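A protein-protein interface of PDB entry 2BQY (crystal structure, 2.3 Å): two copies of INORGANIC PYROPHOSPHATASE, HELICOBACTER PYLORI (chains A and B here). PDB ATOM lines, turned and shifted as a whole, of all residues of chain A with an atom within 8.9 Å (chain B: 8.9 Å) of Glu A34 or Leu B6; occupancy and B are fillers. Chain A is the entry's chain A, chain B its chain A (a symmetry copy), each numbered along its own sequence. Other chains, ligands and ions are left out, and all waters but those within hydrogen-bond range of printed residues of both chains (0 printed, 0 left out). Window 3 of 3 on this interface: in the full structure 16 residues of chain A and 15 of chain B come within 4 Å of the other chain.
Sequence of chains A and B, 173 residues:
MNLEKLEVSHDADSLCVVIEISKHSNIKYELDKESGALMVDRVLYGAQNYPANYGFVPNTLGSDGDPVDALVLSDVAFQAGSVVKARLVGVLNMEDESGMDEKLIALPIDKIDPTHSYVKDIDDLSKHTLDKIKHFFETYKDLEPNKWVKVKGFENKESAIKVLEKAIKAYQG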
ATOM      1  N   GLU A   4      35.473 -19.381 -29.764  1.00  0.00           N
ATOM      2  CA  GLU A   4      35.967 -19.872 -28.449  1.00  0.00           C
ATOM      3  C   GLU A   4      36.888 -21.082 -28.663  1.00  0.00           C
ATOM      4  O   GLU A   4      38.113 -20.955 -28.698  1.00  0.00           O
ATOM      5  CB  GLU A   4      34.790 -20.277 -27.562  1.00  0.00           C
ATOM      6  CG  GLU A   4      35.065 -20.158 -26.050  1.00  0.00           C
ATOM      7  CD  GLU A   4      34.032 -20.943 -25.205  1.00  0.00           C
ATOM      8  OE1 GLU A   4      34.059 -22.225 -25.280  1.00  0.00           O
ATOM      9  OE2 GLU A   4      33.209 -20.263 -24.495  1.00  0.00           O
ATOM     10  N   LYS A   5      36.287 -22.261 -28.843  1.00  0.00           N
ATOM     11  CA  LYS A   5      37.039 -23.509 -29.041  1.00  0.00           C
ATOM     12  C   LYS A   5      38.120 -23.521 -30.128  1.00  0.00           C
ATOM     13  O   LYS A   5      37.824 -23.738 -31.311  1.00  0.00           O
ATOM     14  CB  LYS A   5      36.074 -24.679 -29.294  1.00  0.00           C
ATOM     15  CG  LYS A   5      35.212 -25.013 -28.062  1.00  0.00           C
ATOM     16  CD  LYS A   5      33.769 -25.282 -28.454  1.00  0.00           C
ATOM     17  CE  LYS A   5      33.677 -26.315 -29.592  1.00  0.00           C
ATOM     18  NZ  LYS A   5      34.444 -27.529 -29.244  1.00  0.00           N
ATOM     19  N   LEU A  31      26.809 -28.043 -26.095  1.00  0.00           N
ATOM     20  CA  LEU A  31      27.434 -26.870 -26.692  1.00  0.00           C
ATOM     21  C   LEU A  31      27.295 -26.797 -28.209  1.00  0.00           C
ATOM     22  O   LEU A  31      27.622 -27.744 -28.927  1.00  0.00           O
ATOM     23  CB  LEU A  31      28.917 -26.827 -26.312  1.00  0.00           C
ATOM     24  CG  LEU A  31      29.700 -25.593 -26.759  1.00  0.00           C
ATOM     25  CD1 LEU A  31      29.081 -24.338 -26.145  1.00  0.00           C
ATOM     26  CD2 LEU A  31      31.140 -25.723 -26.319  1.00  0.00           C
ATOM     27  N   ASP A  32      26.775 -25.666 -28.682  1.00  0.00           N
ATOM     28  CA  ASP A  32      26.606 -25.408 -30.106  1.00  0.00           C
ATOM     29  C   ASP A  32      27.898 -24.756 -30.607  1.00  0.00           C
ATOM     30  O   ASP A  32      28.025 -23.535 -30.615  1.00  0.00           O
ATOM     31  CB  ASP A  32      25.448 -24.451 -30.304  1.00  0.00           C
ATOM     32  CG  ASP A  32      25.257 -24.057 -31.766  1.00  0.00           C
ATOM     33  OD1 ASP A  32      24.880 -24.954 -32.583  1.00  0.00           O
ATOM     34  OD2 ASP A  32      25.483 -22.848 -32.075  1.00  0.00           O
ATOM     35  N   LYS A  33      28.853 -25.586 -31.014  1.00  0.00           N
ATOM     36  CA  LYS A  33      30.165 -25.128 -31.467  1.00  0.00           C
ATOM     37  C   LYS A  33      30.193 -23.848 -32.296  1.00  0.00           C
ATOM     38  O   LYS A  33      31.143 -23.032 -32.161  1.00  0.00           O
ATOM     39  CB  LYS A  33      30.879 -26.234 -32.240  1.00  0.00           C
ATOM     40  CG  LYS A  33      32.264 -25.818 -32.719  1.00  0.00           C
ATOM     41  CD  LYS A  33      33.160 -27.032 -32.982  1.00  0.00           C
ATOM     42  CE  LYS A  33      34.565 -26.580 -33.442  1.00  0.00           C
ATOM     43  NZ  LYS A  33      35.556 -27.725 -33.464  1.00  0.00           N
ATOM     44  N   GLU A  34      29.182 -23.669 -33.150  1.00  0.00           N
ATOM     45  CA  GLU A  34      29.144 -22.473 -33.990  1.00  0.00           C
ATOM     46  C   GLU A  34      28.901 -21.188 -33.179  1.00  0.00           C
ATOM     47  O   GLU A  34      29.618 -20.166 -33.375  1.00  0.00           O
ATOM     48  CB  GLU A  34      28.074 -22.609 -35.075  1.00  0.00           C
ATOM     49  CG  GLU A  34      26.792 -23.225 -34.567  1.00  0.00           C
ATOM     50  CD  GLU A  34      25.561 -22.704 -35.313  1.00  0.00           C
ATOM     51  OE1 GLU A  34      25.484 -22.882 -36.560  1.00  0.00           O
ATOM     52  OE2 GLU A  34      24.674 -22.106 -34.648  1.00  0.00           O
ATOM     53  N   SER A  35      27.913 -21.247 -32.283  1.00  0.00           N
ATOM     54  CA  SER A  35      27.572 -20.090 -31.463  1.00  0.00           C
ATOM     55  C   SER A  35      28.352 -20.066 -30.156  1.00  0.00           C
ATOM     56  O   SER A  35      28.573 -19.004 -29.559  1.00  0.00           O
ATOM     57  CB  SER A  35      26.080 -20.089 -31.158  1.00  0.00           C
ATOM     58  OG  SER A  35      25.314 -20.162 -32.355  1.00  0.00           O
ATOM     59  N   GLY A  36      28.788 -21.242 -29.720  1.00  0.00           N
ATOM     60  CA  GLY A  36      29.520 -21.324 -28.471  1.00  0.00           C
ATOM     61  C   GLY A  36      28.507 -21.172 -27.348  1.00  0.00           C
ATOM     62  O   GLY A  36      28.872 -21.018 -26.173  1.00  0.00           O
ATOM     63  N   ALA A  37      27.228 -21.213 -27.717  1.00  0.00           N
ATOM     64  CA  ALA A  37      26.136 -21.057 -26.763  1.00  0.00           C
ATOM     65  C   ALA A  37      25.814 -22.379 -26.074  1.00  0.00           C
ATOM     66  O   ALA A  37      25.635 -23.412 -26.735  1.00  0.00           O
ATOM     67  CB  ALA A  37      24.890 -20.520 -27.482  1.00  0.00           C
ATOM     68  N   MET A  39      23.596 -24.840 -24.803  1.00  0.00           N
ATOM     69  CA  MET A  39      22.201 -25.193 -25.060  1.00  0.00           C
ATOM     70  C   MET A  39      21.610 -26.157 -24.032  1.00  0.00           C
ATOM     71  O   MET A  39      22.256 -27.110 -23.616  1.00  0.00           O
ATOM     72  CB  MET A  39      22.092 -25.830 -26.450  1.00  0.00           C
ATOM     73  CG  MET A  39      21.164 -25.137 -27.408  1.00  0.00           C
ATOM     74  SD  MET A  39      21.656 -23.434 -27.780  1.00  0.00           S
ATOM     75  CE  MET A  39      20.050 -22.720 -28.146  1.00  0.00           C
ATOM     76  N   PHE A  56      32.758 -33.520 -23.864  1.00  0.00           N
ATOM     77  CA  PHE A  56      33.219 -34.076 -25.129  1.00  0.00           C
ATOM     78  C   PHE A  56      34.622 -33.593 -25.462  1.00  0.00           C
ATOM     79  O   PHE A  56      35.041 -32.539 -25.003  1.00  0.00           O
ATOM     80  CB  PHE A  56      32.257 -33.677 -26.261  1.00  0.00           C
ATOM     81  CG  PHE A  56      32.318 -32.219 -26.631  1.00  0.00           C
ATOM     82  CD1 PHE A  56      33.288 -31.749 -27.519  1.00  0.00           C
ATOM     83  CD2 PHE A  56      31.412 -31.314 -26.090  1.00  0.00           C
ATOM     84  CE1 PHE A  56      33.357 -30.395 -27.871  1.00  0.00           C
ATOM     85  CE2 PHE A  56      31.474 -29.951 -26.438  1.00  0.00           C
ATOM     86  CZ  PHE A  56      32.453 -29.496 -27.329  1.00  0.00           C
ATOM     87  N   GLU B   4      28.765 -14.933 -30.411  1.00  0.00           N
ATOM     88  CA  GLU B   4      27.988 -16.059 -29.824  1.00  0.00           C
ATOM     89  C   GLU B   4      26.567 -16.066 -30.407  1.00  0.00           C
ATOM     90  O   GLU B   4      26.269 -16.795 -31.353  1.00  0.00           O
ATOM     91  CB  GLU B   4      27.916 -15.913 -28.304  1.00  0.00           C
ATOM     92  CG  GLU B   4      27.762 -17.246 -27.545  1.00  0.00           C
ATOM     93  CD  GLU B   4      27.290 -17.036 -26.085  1.00  0.00           C
ATOM     94  OE1 GLU B   4      26.094 -16.602 -25.907  1.00  0.00           O
ATOM     95  OE2 GLU B   4      28.128 -17.296 -25.149  1.00  0.00           O
ATOM     96  N   LYS B   5      25.696 -15.218 -29.854  1.00  0.00           N
ATOM     97  CA  LYS B   5      24.296 -15.126 -30.296  1.00  0.00           C
ATOM     98  C   LYS B   5      24.035 -14.938 -31.795  1.00  0.00           C
ATOM     99  O   LYS B   5      24.068 -13.810 -32.305  1.00  0.00           O
ATOM    100  CB  LYS B   5      23.565 -14.014 -29.526  1.00  0.00           C
ATOM    101  CG  LYS B   5      23.413 -14.331 -28.027  1.00  0.00           C
ATOM    102  CD  LYS B   5      23.703 -13.111 -27.170  1.00  0.00           C
ATOM    103  CE  LYS B   5      22.899 -11.886 -27.644  1.00  0.00           C
ATOM    104  NZ  LYS B   5      21.464 -12.223 -27.747  1.00  0.00           N
ATOM    105  N   LEU B   6      23.780 -16.055 -32.478  1.00  0.00           N
ATOM    106  CA  LEU B   6      23.455 -16.084 -33.912  1.00  0.00           C
ATOM    107  C   LEU B   6      22.842 -17.463 -34.162  1.00  0.00           C
ATOM    108  O   LEU B   6      23.596 -18.405 -34.474  1.00  0.00           O
ATOM    109  CB  LEU B   6      24.711 -15.924 -34.792  1.00  0.00           C
ATOM    110  CG  LEU B   6      25.377 -14.552 -34.921  1.00  0.00           C
ATOM    111  CD1 LEU B   6      26.442 -14.371 -33.838  1.00  0.00           C
ATOM    112  CD2 LEU B   6      26.028 -14.465 -36.309  1.00  0.00           C
ATOM    113  N   GLU B   7      21.516 -17.586 -34.014  1.00  0.00           N
ATOM    114  CA  GLU B   7      20.855 -18.880 -34.186  1.00  0.00           C
ATOM    115  C   GLU B   7      19.330 -18.746 -34.253  1.00  0.00           C
ATOM    116  O   GLU B   7      18.650 -19.464 -35.000  1.00  0.00           O
ATOM    117  CB  GLU B   7      21.198 -19.766 -32.985  1.00  0.00           C
ATOM    118  CG  GLU B   7      20.360 -19.415 -31.701  1.00  0.00           C
ATOM    119  CD  GLU B   7      21.201 -19.093 -30.463  1.00  0.00           C
ATOM    120  OE1 GLU B   7      22.062 -19.936 -30.111  1.00  0.00           O
ATOM    121  OE2 GLU B   7      20.983 -18.012 -29.849  1.00  0.00           O
ATOM    122  N   VAL B   8      18.822 -17.840 -33.413  1.00  0.00           N
ATOM    123  CA  VAL B   8      17.402 -17.532 -33.236  1.00  0.00           C
ATOM    124  C   VAL B   8      16.285 -18.264 -33.986  1.00  0.00           C
ATOM    125  O   VAL B   8      16.254 -18.361 -35.223  1.00  0.00           O
ATOM    126  CB  VAL B   8      17.140 -16.035 -33.429  1.00  0.00           C
ATOM    127  CG1 VAL B   8      15.743 -15.693 -32.885  1.00  0.00           C
ATOM    128  CG2 VAL B   8      18.224 -15.215 -32.692  1.00  0.00           C
ATOM    129  N   SER B   9      15.354 -18.756 -33.174  1.00  0.00           N
ATOM    130  CA  SER B   9      14.153 -19.438 -33.632  1.00  0.00           C
ATOM    131  C   SER B   9      13.083 -18.525 -33.021  1.00  0.00           C
ATOM    132  O   SER B   9      13.186 -18.161 -31.828  1.00  0.00           O
ATOM    133  CB  SER B   9      14.028 -20.838 -33.019  1.00  0.00           C
ATOM    134  OG  SER B   9      12.737 -21.384 -33.288  1.00  0.00           O
ATOM    135  N   CYS B  16      13.512 -19.413 -28.555  1.00  0.00           N
ATOM    136  CA  CYS B  16      14.595 -19.611 -27.595  1.00  0.00           C
ATOM    137  C   CYS B  16      14.754 -18.423 -26.646  1.00  0.00           C
ATOM    138  O   CYS B  16      14.603 -17.259 -27.049  1.00  0.00           O
ATOM    139  CB  CYS B  16      15.924 -19.882 -28.317  1.00  0.00           C
ATOM    140  SG  CYS B  16      16.680 -18.442 -28.976  1.00  0.00           S
ATOM    141  N   VAL B  18      17.316 -16.651 -23.700  1.00  0.00           N
ATOM    142  CA  VAL B  18      18.675 -16.610 -23.178  1.00  0.00           C
ATOM    143  C   VAL B  18      18.601 -16.334 -21.677  1.00  0.00           C
ATOM    144  O   VAL B  18      18.296 -15.229 -21.257  1.00  0.00           O
ATOM    145  CB  VAL B  18      19.516 -15.502 -23.873  1.00  0.00           C
ATOM    146  CG1 VAL B  18      20.927 -15.483 -23.317  1.00  0.00           C
ATOM    147  CG2 VAL B  18      19.543 -15.733 -25.369  1.00  0.00           C
ATOM    148  N   LYS B  33      25.398  -8.220 -25.165  1.00  0.00           N
ATOM    149  CA  LYS B  33      25.424  -8.789 -26.512  1.00  0.00           C
ATOM    150  C   LYS B  33      26.701  -8.574 -27.319  1.00  0.00           C
ATOM    151  O   LYS B  33      27.120  -9.482 -28.086  1.00  0.00           O
ATOM    152  CB  LYS B  33      24.235  -8.286 -27.327  1.00  0.00           C
ATOM    153  CG  LYS B  33      24.200  -8.863 -28.736  1.00  0.00           C
ATOM    154  CD  LYS B  33      22.790  -8.818 -29.331  1.00  0.00           C
ATOM    155  CE  LYS B  33      22.781  -9.432 -30.750  1.00  0.00           C
ATOM    156  NZ  LYS B  33      21.374  -9.644 -31.272  1.00  0.00           N
ATOM    157  N   PRO B  58      16.258 -13.240 -28.001  1.00  0.00           N
ATOM    158  CA  PRO B  58      17.161 -12.504 -28.891  1.00  0.00           C
ATOM    159  C   PRO B  58      16.524 -12.088 -30.211  1.00  0.00           C
ATOM    160  O   PRO B  58      15.576 -12.716 -30.675  1.00  0.00           O
ATOM    161  CB  PRO B  58      18.325 -13.475 -29.079  1.00  0.00           C
ATOM    162  CG  PRO B  58      17.637 -14.805 -29.041  1.00  0.00           C
ATOM    163  CD  PRO B  58      16.674 -14.648 -27.878  1.00  0.00           C
ATOM    164  N   ASN B  59      17.059 -11.025 -30.806  1.00  0.00           N
ATOM    165  CA  ASN B  59      16.566 -10.509 -32.083  1.00  0.00           C
ATOM    166  C   ASN B  59      15.138  -9.971 -32.009  1.00  0.00           C
ATOM    167  O   ASN B  59      14.345 -10.156 -32.923  1.00  0.00           O
ATOM    168  CB  ASN B  59      16.666 -11.589 -33.163  1.00  0.00           C
ATOM    169  CG  ASN B  59      18.080 -11.976 -33.455  1.00  0.00           C
ATOM    170  OD1 ASN B  59      18.327 -12.818 -34.300  1.00  0.00           O
ATOM    171  ND2 ASN B  59      19.023 -11.366 -32.752  1.00  0.00           N
ATOM    172  N   VAL B  83      20.999 -21.265 -23.033  1.00  0.00           N
ATOM    173  CA  VAL B  83      19.854 -20.960 -23.874  1.00  0.00           C
ATOM    174  C   VAL B  83      18.883 -22.110 -23.806  1.00  0.00           C
ATOM    175  O   VAL B  83      19.286 -23.259 -23.804  1.00  0.00           O
ATOM    176  CB  VAL B  83      20.279 -20.737 -25.352  1.00  0.00           C
ATOM    177  CG1 VAL B  83      19.093 -20.184 -26.157  1.00  0.00           C
ATOM    178  CG2 VAL B  83      21.460 -19.773 -25.420  1.00  0.00           C
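The side-chain hydroxyl of Ser A35 is in hydrogen-bond range of the backbone carbonyl oxygen of Leu B6 (3.2 Å).
The side-chain carboxylate of Asp A32 sits at hydrogen-bond distance from the side-chain hydroxyl of Ser A35 (2.7 Å).
The side-chain hydroxyl of Ser A35 lies within hydrogen-bond range of the side-chain carboxylate of Glu A34.
The backbone carbonyl oxygen of Ala A37 is in hydrogen-bond range of the backbone NH of Asp A32 (3.2 Å).
O of Leu B6 touches OE2 of Glu A34, at 3.9 Å.
Ser A35 touches Glu B4 (O to CG, 2.8 Å).
Glu B7 touches Ser A35.
OE2 of Glu B4 touches O of Gly A36, 3.9 Å away.
Ala A37 touches Glu B7.
Met A39 touches Glu B7 (CE to OE1, 3.96 Å).
Val B83 touches Met A39.
Glu A34 touches one residue of chain B.
Of chain A, only Glu A34 and Ser A35 come within 4 Å of Leu B6.
Ser A35 touches just these residues of chain B: Glu B4, Leu B6 and Glu B7.
Of chain A, only Ser A35, Ala A37 and Met A39 come within 4 Å of Glu B7.
Printed residues of chain A within 4 Å of Val B83: Met A39.
Of the printed residues of chain B, Met A39 touches Glu B7 and Val B83.
Printed residues of chain A within 4 Å of Glu B4: Ser A35 (2.8 Å) and Gly A36 (3.9 Å).
Of the printed residues of chain B, Ala A37 touches Glu B7.
The nearest residue of chain A that does not touch Leu B6 is Asp A32 (5.4 Å).
Of the 12 printed residues of chain B, 4 touch a printed residue of chain A.
Among the printed residues, no Asp or Glu carboxylate lies within 4 Å of a Lys or Arg side-chain nitrogen of the other chain.
Positions printed for both chains: 4, 5 and 33.
Of the 8 pairs that touch across the chains among the printed residues, none has its exchanged pair printed and touching as well.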
